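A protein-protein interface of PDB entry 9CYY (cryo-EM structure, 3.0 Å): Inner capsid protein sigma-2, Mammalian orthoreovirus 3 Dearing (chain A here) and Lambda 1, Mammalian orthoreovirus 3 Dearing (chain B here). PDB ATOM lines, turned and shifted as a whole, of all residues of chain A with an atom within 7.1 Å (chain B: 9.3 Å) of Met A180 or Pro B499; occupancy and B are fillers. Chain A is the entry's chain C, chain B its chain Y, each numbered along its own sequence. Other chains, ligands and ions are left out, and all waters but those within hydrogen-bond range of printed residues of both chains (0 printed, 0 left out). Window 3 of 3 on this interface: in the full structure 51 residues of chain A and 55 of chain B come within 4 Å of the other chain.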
ATOM      1  N   ASP A 174      16.918  -4.931  -1.233  1.00  0.00           N
ATOM      2  CA  ASP A 174      15.498  -5.054  -1.541  1.00  0.00           C
ATOM      3  C   ASP A 174      15.245  -6.187  -2.525  1.00  0.00           C
ATOM      4  O   ASP A 174      14.254  -6.917  -2.404  1.00  0.00           O
ATOM      5  CB  ASP A 174      14.963  -3.731  -2.087  1.00  0.00           C
ATOM      6  CG  ASP A 174      15.780  -3.207  -3.248  1.00  0.00           C
ATOM      7  OD1 ASP A 174      16.811  -3.829  -3.579  1.00  0.00           O
ATOM      8  OD2 ASP A 174      15.391  -2.173  -3.831  1.00  0.00           O
ATOM      9  N   VAL A 175      16.134  -6.350  -3.508  1.00  0.00           N
ATOM     10  CA  VAL A 175      15.987  -7.440  -4.467  1.00  0.00           C
ATOM     11  C   VAL A 175      16.086  -8.784  -3.763  1.00  0.00           C
ATOM     12  O   VAL A 175      15.300  -9.697  -4.033  1.00  0.00           O
ATOM     13  CB  VAL A 175      17.031  -7.310  -5.591  1.00  0.00           C
ATOM     14  CG1 VAL A 175      16.914  -8.473  -6.555  1.00  0.00           C
ATOM     15  CG2 VAL A 175      16.848  -5.997  -6.324  1.00  0.00           C
ATOM     16  N   ASN A 176      17.051  -8.931  -2.853  1.00  0.00           N
ATOM     17  CA  ASN A 176      17.172 -10.177  -2.103  1.00  0.00           C
ATOM     18  C   ASN A 176      15.929 -10.438  -1.265  1.00  0.00           C
ATOM     19  O   ASN A 176      15.407 -11.562  -1.243  1.00  0.00           O
ATOM     20  CB  ASN A 176      18.411 -10.135  -1.210  1.00  0.00           C
ATOM     21  CG  ASN A 176      19.685 -10.429  -1.967  1.00  0.00           C
ATOM     22  OD1 ASN A 176      19.903 -11.549  -2.424  1.00  0.00           O
ATOM     23  ND2 ASN A 176      20.538  -9.423  -2.100  1.00  0.00           N
ATOM     24  N   GLN A 177      15.437  -9.407  -0.575  1.00  0.00           N
ATOM     25  CA  GLN A 177      14.269  -9.577   0.281  1.00  0.00           C
ATOM     26  C   GLN A 177      13.048  -9.990  -0.527  1.00  0.00           C
ATOM     27  O   GLN A 177      12.285 -10.868  -0.109  1.00  0.00           O
ATOM     28  CB  GLN A 177      13.990  -8.287   1.049  1.00  0.00           C
ATOM     29  CG  GLN A 177      12.819  -8.385   2.005  1.00  0.00           C
ATOM     30  CD  GLN A 177      12.564  -7.091   2.746  1.00  0.00           C
ATOM     31  OE1 GLN A 177      13.244  -6.091   2.523  1.00  0.00           O
ATOM     32  NE2 GLN A 177      11.578  -7.103   3.635  1.00  0.00           N
ATOM     33  N   LEU A 178      12.844  -9.368  -1.689  1.00  0.00           N
ATOM     34  CA  LEU A 178      11.698  -9.723  -2.517  1.00  0.00           C
ATOM     35  C   LEU A 178      11.861 -11.110  -3.128  1.00  0.00           C
ATOM     36  O   LEU A 178      10.896 -11.878  -3.200  1.00  0.00           O
ATOM     37  CB  LEU A 178      11.493  -8.675  -3.607  1.00  0.00           C
ATOM     38  CG  LEU A 178      10.112  -8.671  -4.262  1.00  0.00           C
ATOM     39  CD1 LEU A 178       9.024  -8.695  -3.207  1.00  0.00           C
ATOM     40  CD2 LEU A 178       9.958  -7.458  -5.160  1.00  0.00           C
ATOM     41  N   LEU A 179      13.073 -11.448  -3.574  1.00  0.00           N
ATOM     42  CA  LEU A 179      13.294 -12.735  -4.223  1.00  0.00           C
ATOM     43  C   LEU A 179      13.116 -13.887  -3.248  1.00  0.00           C
ATOM     44  O   LEU A 179      12.651 -14.966  -3.633  1.00  0.00           O
ATOM     45  CB  LEU A 179      14.688 -12.776  -4.843  1.00  0.00           C
ATOM     46  CG  LEU A 179      14.967 -13.957  -5.769  1.00  0.00           C
ATOM     47  CD1 LEU A 179      14.013 -13.947  -6.946  1.00  0.00           C
ATOM     48  CD2 LEU A 179      16.406 -13.930  -6.243  1.00  0.00           C
ATOM     49  N   MET A 180      13.487 -13.684  -1.983  1.00  0.00           N
ATOM     50  CA  MET A 180      13.416 -14.781  -1.027  1.00  0.00           C
ATOM     51  C   MET A 180      11.985 -15.259  -0.806  1.00  0.00           C
ATOM     52  O   MET A 180      11.779 -16.398  -0.374  1.00  0.00           O
ATOM     53  CB  MET A 180      14.043 -14.351   0.300  1.00  0.00           C
ATOM     54  CG  MET A 180      14.169 -15.469   1.304  1.00  0.00           C
ATOM     55  SD  MET A 180      15.341 -16.682   0.678  1.00  0.00           S
ATOM     56  CE  MET A 180      14.819 -18.141   1.556  1.00  0.00           C
ATOM     57  N   ASN A 181      10.991 -14.425  -1.116  1.00  0.00           N
ATOM     58  CA  ASN A 181       9.595 -14.766  -0.874  1.00  0.00           C
ATOM     59  C   ASN A 181       9.039 -15.784  -1.861  1.00  0.00           C
ATOM     60  O   ASN A 181       7.971 -16.344  -1.601  1.00  0.00           O
ATOM     61  CB  ASN A 181       8.736 -13.502  -0.910  1.00  0.00           C
ATOM     62  CG  ASN A 181       8.768 -12.740   0.394  1.00  0.00           C
ATOM     63  OD1 ASN A 181       9.300 -11.634   0.466  1.00  0.00           O
ATOM     64  ND2 ASN A 181       8.197 -13.327   1.435  1.00  0.00           N
ATOM     65  N   TYR A 182       9.719 -16.035  -2.976  1.00  0.00           N
ATOM     66  CA  TYR A 182       9.243 -16.957  -4.001  1.00  0.00           C
ATOM     67  C   TYR A 182       9.965 -18.298  -3.916  1.00  0.00           C
ATOM     68  O   TYR A 182      10.259 -18.926  -4.933  1.00  0.00           O
ATOM     69  CB  TYR A 182       9.420 -16.361  -5.393  1.00  0.00           C
ATOM     70  CG  TYR A 182       8.688 -15.060  -5.611  1.00  0.00           C
ATOM     71  CD1 TYR A 182       7.337 -15.044  -5.919  1.00  0.00           C
ATOM     72  CD2 TYR A 182       9.355 -13.848  -5.526  1.00  0.00           C
ATOM     73  CE1 TYR A 182       6.667 -13.856  -6.122  1.00  0.00           C
ATOM     74  CE2 TYR A 182       8.695 -12.655  -5.729  1.00  0.00           C
ATOM     75  CZ  TYR A 182       7.353 -12.665  -6.027  1.00  0.00           C
ATOM     76  OH  TYR A 182       6.691 -11.476  -6.230  1.00  0.00           O
ATOM     77  N   PHE A 183      10.251 -18.750  -2.694  1.00  0.00           N
ATOM     78  CA  PHE A 183      11.110 -19.917  -2.519  1.00  0.00           C
ATOM     79  C   PHE A 183      10.492 -21.171  -3.121  1.00  0.00           C
ATOM     80  O   PHE A 183      11.190 -21.965  -3.761  1.00  0.00           O
ATOM     81  CB  PHE A 183      11.407 -20.129  -1.036  1.00  0.00           C
ATOM     82  CG  PHE A 183      11.985 -21.477  -0.723  1.00  0.00           C
ATOM     83  CD1 PHE A 183      13.154 -21.900  -1.327  1.00  0.00           C
ATOM     84  CD2 PHE A 183      11.354 -22.324   0.170  1.00  0.00           C
ATOM     85  CE1 PHE A 183      13.684 -23.139  -1.042  1.00  0.00           C
ATOM     86  CE2 PHE A 183      11.881 -23.564   0.456  1.00  0.00           C
ATOM     87  CZ  PHE A 183      13.047 -23.971  -0.150  1.00  0.00           C
ATOM     88  N   GLY A 184       9.193 -21.374  -2.934  1.00  0.00           N
ATOM     89  CA  GLY A 184       8.589 -22.622  -3.359  1.00  0.00           C
ATOM     90  C   GLY A 184       7.609 -22.516  -4.509  1.00  0.00           C
ATOM     91  O   GLY A 184       6.982 -23.510  -4.882  1.00  0.00           O
ATOM     92  N   MET A 212      14.470  -7.547 -10.556  1.00  0.00           N
ATOM     93  CA  MET A 212      14.118  -8.903 -10.159  1.00  0.00           C
ATOM     94  C   MET A 212      13.585  -9.701 -11.342  1.00  0.00           C
ATOM     95  O   MET A 212      13.840 -10.903 -11.458  1.00  0.00           O
ATOM     96  CB  MET A 212      13.100  -8.877  -9.021  1.00  0.00           C
ATOM     97  CG  MET A 212      12.731 -10.260  -8.518  1.00  0.00           C
ATOM     98  SD  MET A 212      11.553 -10.231  -7.162  1.00  0.00           S
ATOM     99  CE  MET A 212      10.070  -9.740  -8.031  1.00  0.00           C
ATOM    100  N   PHE A 237      20.587 -20.201  -5.854  1.00  0.00           N
ATOM    101  CA  PHE A 237      19.272 -20.176  -6.478  1.00  0.00           C
ATOM    102  C   PHE A 237      19.313 -20.963  -7.779  1.00  0.00           C
ATOM    103  O   PHE A 237      20.285 -20.875  -8.533  1.00  0.00           O
ATOM    104  CB  PHE A 237      18.812 -18.744  -6.757  1.00  0.00           C
ATOM    105  CG  PHE A 237      18.254 -18.041  -5.556  1.00  0.00           C
ATOM    106  CD1 PHE A 237      16.974 -18.314  -5.113  1.00  0.00           C
ATOM    107  CD2 PHE A 237      19.005 -17.100  -4.878  1.00  0.00           C
ATOM    108  CE1 PHE A 237      16.456 -17.665  -4.013  1.00  0.00           C
ATOM    109  CE2 PHE A 237      18.492 -16.450  -3.777  1.00  0.00           C
ATOM    110  CZ  PHE A 237      17.217 -16.733  -3.343  1.00  0.00           C
ATOM    111  N   LEU A 253      11.314 -22.822  -8.363  1.00  0.00           N
ATOM    112  CA  LEU A 253      12.462 -22.144  -7.783  1.00  0.00           C
ATOM    113  C   LEU A 253      12.928 -22.889  -6.536  1.00  0.00           C
ATOM    114  O   LEU A 253      12.126 -23.456  -5.793  1.00  0.00           O
ATOM    115  CB  LEU A 253      12.110 -20.699  -7.437  1.00  0.00           C
ATOM    116  CG  LEU A 253      13.276 -19.771  -7.098  1.00  0.00           C
ATOM    117  CD1 LEU A 253      14.280 -19.751  -8.230  1.00  0.00           C
ATOM    118  CD2 LEU A 253      12.778 -18.370  -6.808  1.00  0.00           C
ATOM    119  N   CYS A 255      16.517 -23.273  -3.538  1.00  0.00           N
ATOM    120  CA  CYS A 255      17.782 -22.825  -2.977  1.00  0.00           C
ATOM    121  C   CYS A 255      18.580 -24.033  -2.517  1.00  0.00           C
ATOM    122  O   CYS A 255      18.007 -25.041  -2.095  1.00  0.00           O
ATOM    123  CB  CYS A 255      17.570 -21.871  -1.797  1.00  0.00           C
ATOM    124  SG  CYS A 255      16.392 -20.543  -2.104  1.00  0.00           S
ATOM    125  N   MET B 439       9.424 -29.502  -0.558  1.00  0.00           N
ATOM    126  CA  MET B 439      10.330 -28.370  -0.453  1.00  0.00           C
ATOM    127  C   MET B 439      11.044 -28.295   0.891  1.00  0.00           C
ATOM    128  O   MET B 439      12.020 -27.550   1.015  1.00  0.00           O
ATOM    129  CB  MET B 439       9.570 -27.066  -0.709  1.00  0.00           C
ATOM    130  CG  MET B 439       9.120 -26.894  -2.150  1.00  0.00           C
ATOM    131  SD  MET B 439      10.461 -26.976  -3.348  1.00  0.00           S
ATOM    132  CE  MET B 439      11.526 -25.669  -2.759  1.00  0.00           C
ATOM    133  N   MET B 440      10.585 -29.037   1.896  1.00  0.00           N
ATOM    134  CA  MET B 440      11.223 -29.026   3.207  1.00  0.00           C
ATOM    135  C   MET B 440      11.122 -30.406   3.831  1.00  0.00           C
ATOM    136  O   MET B 440      10.281 -31.220   3.438  1.00  0.00           O
ATOM    137  CB  MET B 440      10.595 -27.989   4.146  1.00  0.00           C
ATOM    138  CG  MET B 440      10.822 -26.548   3.749  1.00  0.00           C
ATOM    139  SD  MET B 440      10.043 -25.419   4.908  1.00  0.00           S
ATOM    140  CE  MET B 440      10.398 -23.850   4.135  1.00  0.00           C
ATOM    141  N   GLU B 446       4.106 -29.411  -0.933  1.00  0.00           N
ATOM    142  CA  GLU B 446       3.387 -28.245  -1.434  1.00  0.00           C
ATOM    143  C   GLU B 446       2.245 -28.653  -2.356  1.00  0.00           C
ATOM    144  O   GLU B 446       1.143 -28.100  -2.271  1.00  0.00           O
ATOM    145  CB  GLU B 446       4.350 -27.300  -2.150  1.00  0.00           C
ATOM    146  CG  GLU B 446       5.520 -26.835  -1.295  1.00  0.00           C
ATOM    147  CD  GLU B 446       5.105 -25.962  -0.121  1.00  0.00           C
ATOM    148  OE1 GLU B 446       5.976 -25.652   0.719  1.00  0.00           O
ATOM    149  OE2 GLU B 446       3.923 -25.570  -0.039  1.00  0.00           O
ATOM    150  N   ASN B 475       2.493 -11.479  -1.424  1.00  0.00           N
ATOM    151  CA  ASN B 475       3.437 -11.960  -0.423  1.00  0.00           C
ATOM    152  C   ASN B 475       3.643 -10.929   0.683  1.00  0.00           C
ATOM    153  O   ASN B 475       3.382  -9.737   0.495  1.00  0.00           O
ATOM    154  CB  ASN B 475       4.768 -12.316  -1.091  1.00  0.00           C
ATOM    155  CG  ASN B 475       5.524 -11.102  -1.593  1.00  0.00           C
ATOM    156  OD1 ASN B 475       5.979 -10.265  -0.814  1.00  0.00           O
ATOM    157  ND2 ASN B 475       5.665 -11.004  -2.907  1.00  0.00           N
ATOM    158  N   PRO B 476       4.107 -11.365   1.862  1.00  0.00           N
ATOM    159  CA  PRO B 476       4.157 -10.450   3.021  1.00  0.00           C
ATOM    160  C   PRO B 476       5.036  -9.220   2.840  1.00  0.00           C
ATOM    161  O   PRO B 476       4.766  -8.188   3.467  1.00  0.00           O
ATOM    162  CB  PRO B 476       4.686 -11.352   4.142  1.00  0.00           C
ATOM    163  CG  PRO B 476       4.266 -12.715   3.746  1.00  0.00           C
ATOM    164  CD  PRO B 476       4.409 -12.753   2.258  1.00  0.00           C
ATOM    165  N   THR B 477       6.102  -9.304   2.042  1.00  0.00           N
ATOM    166  CA  THR B 477       6.978  -8.147   1.875  1.00  0.00           C
ATOM    167  C   THR B 477       6.239  -6.983   1.228  1.00  0.00           C
ATOM    168  O   THR B 477       6.395  -5.824   1.641  1.00  0.00           O
ATOM    169  CB  THR B 477       8.204  -8.534   1.047  1.00  0.00           C
ATOM    170  OG1 THR B 477       8.920  -9.577   1.718  1.00  0.00           O
ATOM    171  CG2 THR B 477       9.121  -7.342   0.866  1.00  0.00           C
ATOM    172  N   SER B 495       8.471  -8.154   8.498  1.00  0.00           N
ATOM    173  CA  SER B 495       8.159  -9.398   7.819  1.00  0.00           C
ATOM    174  C   SER B 495       9.324 -10.365   7.964  1.00  0.00           C
ATOM    175  O   SER B 495      10.471  -9.939   8.130  1.00  0.00           O
ATOM    176  CB  SER B 495       7.871  -9.157   6.331  1.00  0.00           C
ATOM    177  OG  SER B 495       9.035  -8.717   5.655  1.00  0.00           O
ATOM    178  N   PRO B 496       9.064 -11.667   7.908  1.00  0.00           N
ATOM    179  CA  PRO B 496      10.143 -12.643   8.075  1.00  0.00           C
ATOM    180  C   PRO B 496      11.051 -12.706   6.859  1.00  0.00           C
ATOM    181  O   PRO B 496      10.717 -12.231   5.772  1.00  0.00           O
ATOM    182  CB  PRO B 496       9.397 -13.970   8.269  1.00  0.00           C
ATOM    183  CG  PRO B 496       7.959 -13.602   8.478  1.00  0.00           C
ATOM    184  CD  PRO B 496       7.760 -12.326   7.749  1.00  0.00           C
ATOM    185  N   TYR B 497      12.222 -13.306   7.062  1.00  0.00           N
ATOM    186  CA  TYR B 497      13.213 -13.496   6.005  1.00  0.00           C
ATOM    187  C   TYR B 497      13.773 -14.909   6.141  1.00  0.00           C
ATOM    188  O   TYR B 497      14.773 -15.121   6.832  1.00  0.00           O
ATOM    189  CB  TYR B 497      14.316 -12.447   6.093  1.00  0.00           C
ATOM    190  CG  TYR B 497      15.350 -12.544   4.998  1.00  0.00           C
ATOM    191  CD1 TYR B 497      15.102 -12.028   3.736  1.00  0.00           C
ATOM    192  CD2 TYR B 497      16.577 -13.147   5.227  1.00  0.00           C
ATOM    193  CE1 TYR B 497      16.045 -12.113   2.733  1.00  0.00           C
ATOM    194  CE2 TYR B 497      17.526 -13.237   4.230  1.00  0.00           C
ATOM    195  CZ  TYR B 497      17.255 -12.718   2.986  1.00  0.00           C
ATOM    196  OH  TYR B 497      18.198 -12.806   1.990  1.00  0.00           O
ATOM    197  N   ALA B 498      13.133 -15.866   5.468  1.00  0.00           N
ATOM    198  CA  ALA B 498      13.483 -17.278   5.550  1.00  0.00           C
ATOM    199  C   ALA B 498      12.648 -18.067   4.548  1.00  0.00           C
ATOM    200  O   ALA B 498      11.668 -17.536   4.012  1.00  0.00           O
ATOM    201  CB  ALA B 498      13.261 -17.805   6.970  1.00  0.00           C
ATOM    202  N   PRO B 499      12.999 -19.321   4.256  1.00  0.00           N
ATOM    203  CA  PRO B 499      12.125 -20.145   3.416  1.00  0.00           C
ATOM    204  C   PRO B 499      10.766 -20.347   4.071  1.00  0.00           C
ATOM    205  O   PRO B 499      10.642 -20.382   5.296  1.00  0.00           O
ATOM    206  CB  PRO B 499      12.894 -21.465   3.299  1.00  0.00           C
ATOM    207  CG  PRO B 499      14.311 -21.079   3.483  1.00  0.00           C
ATOM    208  CD  PRO B 499      14.287 -19.988   4.512  1.00  0.00           C
ATOM    209  N   SER B 500       9.736 -20.489   3.235  1.00  0.00           N
ATOM    210  CA  SER B 500       8.366 -20.516   3.734  1.00  0.00           C
ATOM    211  C   SER B 500       7.559 -21.661   3.134  1.00  0.00           C
ATOM    212  O   SER B 500       8.111 -22.527   2.448  1.00  0.00           O
ATOM    213  CB  SER B 500       7.673 -19.184   3.448  1.00  0.00           C
ATOM    214  OG  SER B 500       7.215 -19.125   2.108  1.00  0.00           O
ATOM    215  N   VAL B 501       6.247 -21.666   3.374  1.00  0.00           N
ATOM    216  CA  VAL B 501       5.415 -22.822   3.064  1.00  0.00           C
ATOM    217  C   VAL B 501       4.297 -22.474   2.088  1.00  0.00           C
ATOM    218  O   VAL B 501       3.204 -23.050   2.160  1.00  0.00           O
ATOM    219  CB  VAL B 501       4.834 -23.431   4.352  1.00  0.00           C
ATOM    220  CG1 VAL B 501       5.926 -24.128   5.138  1.00  0.00           C
ATOM    221  CG2 VAL B 501       4.180 -22.352   5.195  1.00  0.00           C
ATOM    222  N   ASN B 502       4.555 -21.536   1.177  1.00  0.00           N
ATOM    223  CA  ASN B 502       3.642 -21.258   0.071  1.00  0.00           C
ATOM    224  C   ASN B 502       2.251 -20.847   0.536  1.00  0.00           C
ATOM    225  O   ASN B 502       1.279 -21.574   0.311  1.00  0.00           O
ATOM    226  CB  ASN B 502       3.538 -22.476  -0.848  1.00  0.00           C
ATOM    227  CG  ASN B 502       4.747 -22.636  -1.741  1.00  0.00           C
ATOM    228  OD1 ASN B 502       5.879 -22.418  -1.315  1.00  0.00           O
ATOM    229  ND2 ASN B 502       4.514 -23.020  -2.989  1.00  0.00           N
ATOM    230  N   ARG B 503       2.143 -19.695   1.189  1.00  0.00           N
ATOM    231  CA  ARG B 503       0.867 -19.167   1.642  1.00  0.00           C
ATOM    232  C   ARG B 503       0.051 -18.689   0.449  1.00  0.00           C
ATOM    233  O   ARG B 503       0.594 -18.414  -0.624  1.00  0.00           O
ATOM    234  CB  ARG B 503       1.066 -18.014   2.625  1.00  0.00           C
ATOM    235  CG  ARG B 503       1.870 -18.392   3.850  1.00  0.00           C
ATOM    236  CD  ARG B 503       2.141 -17.184   4.720  1.00  0.00           C
ATOM    237  NE  ARG B 503       2.934 -17.531   5.890  1.00  0.00           N
ATOM    238  CZ  ARG B 503       4.258 -17.491   5.934  1.00  0.00           C
ATOM    239  NH1 ARG B 503       4.972 -17.118   4.885  1.00  0.00           N
ATOM    240  NH2 ARG B 503       4.881 -17.831   7.058  1.00  0.00           N
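Of the 15 printed residues of chain A, 7 touch a printed residue of chain B. Printed residues of chain A that touch a printed residue of chain B: Gln A177, Met A180, Asn A181, Tyr A182, Phe A183, Gly A184 and Leu A253. Hydrophobic or aromatic side chains of chain A that line the printed part of chain B: Met A180, Tyr A182 and Phe A183. Along chain A the printed residues that touch a printed residue of chain B span positions 177 to 253. Along chain B the printed residues that touch a printed residue of chain A span positions 439 to 502. Among the printed residues, no Asp or Glu carboxylate lies within 4 Å of a Lys or Arg side-chain nitrogen of the other chain.
OD1 of Asn A181 sits close to O of Gln A177. O of Phe A183 lies close to O of Leu A253 (2.7 Å). OD1 of Asn B475 is in hydrogen-bond range of N of Thr B477 (3.0 Å).
Val A175 touches none of the printed residues of chain B. No residue of chain B comes within 4 Å of Leu A179. Met A180 touches just these residues of chain B: Tyr B497, Ala B498 and Pro B499. Of chain B, only Asn B475, Pro B476 and Thr B477 come within 4 Å of Asn A181. Of the printed residues of chain B, Tyr A182 touches Asn B475. Of the printed residues of chain A, Asn B475 touches Asn A181 and Tyr A182. Of the printed residues of chain A, Ser B495 touches Gln A177 (3.6 Å). Pro B499 touches two residues of chain A. Arg B503 touches none of the printed residues of chain A. The nearest residue of chain A that does not touch Pro B499 is Cys A255 (6.0 Å).
OD1 of Asn A181 is in hydrogen-bond range of OG1 of Thr B477 (2.4 Å). The backbone carbonyl oxygen (O) of Gly A184 sits at hydrogen-bond distance from the side-chain amide nitrogen (ND2) of Asn B502.
NE2 of Gln A177 touches CG2 of Thr B477 (3.7 Å). Gln A177 touches Tyr B497. CB of Met A180 touches CE1 of Tyr B497 (3.9 Å). C of Ala B498 touches CE of Met A180, at 3.7 Å. Met A180 touches Pro B499 (CE to N, 3.5 Å). ND2 of Asn A181 touches CD of Pro B476, at 3.9 Å. CE of Met B439 touches CZ of Phe A183 (3.5 Å). CE of Met B440 touches CE2 of Phe A183, at 3.98 Å. Phe A183 touches Pro B499. Leu A253 touches Met B439.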
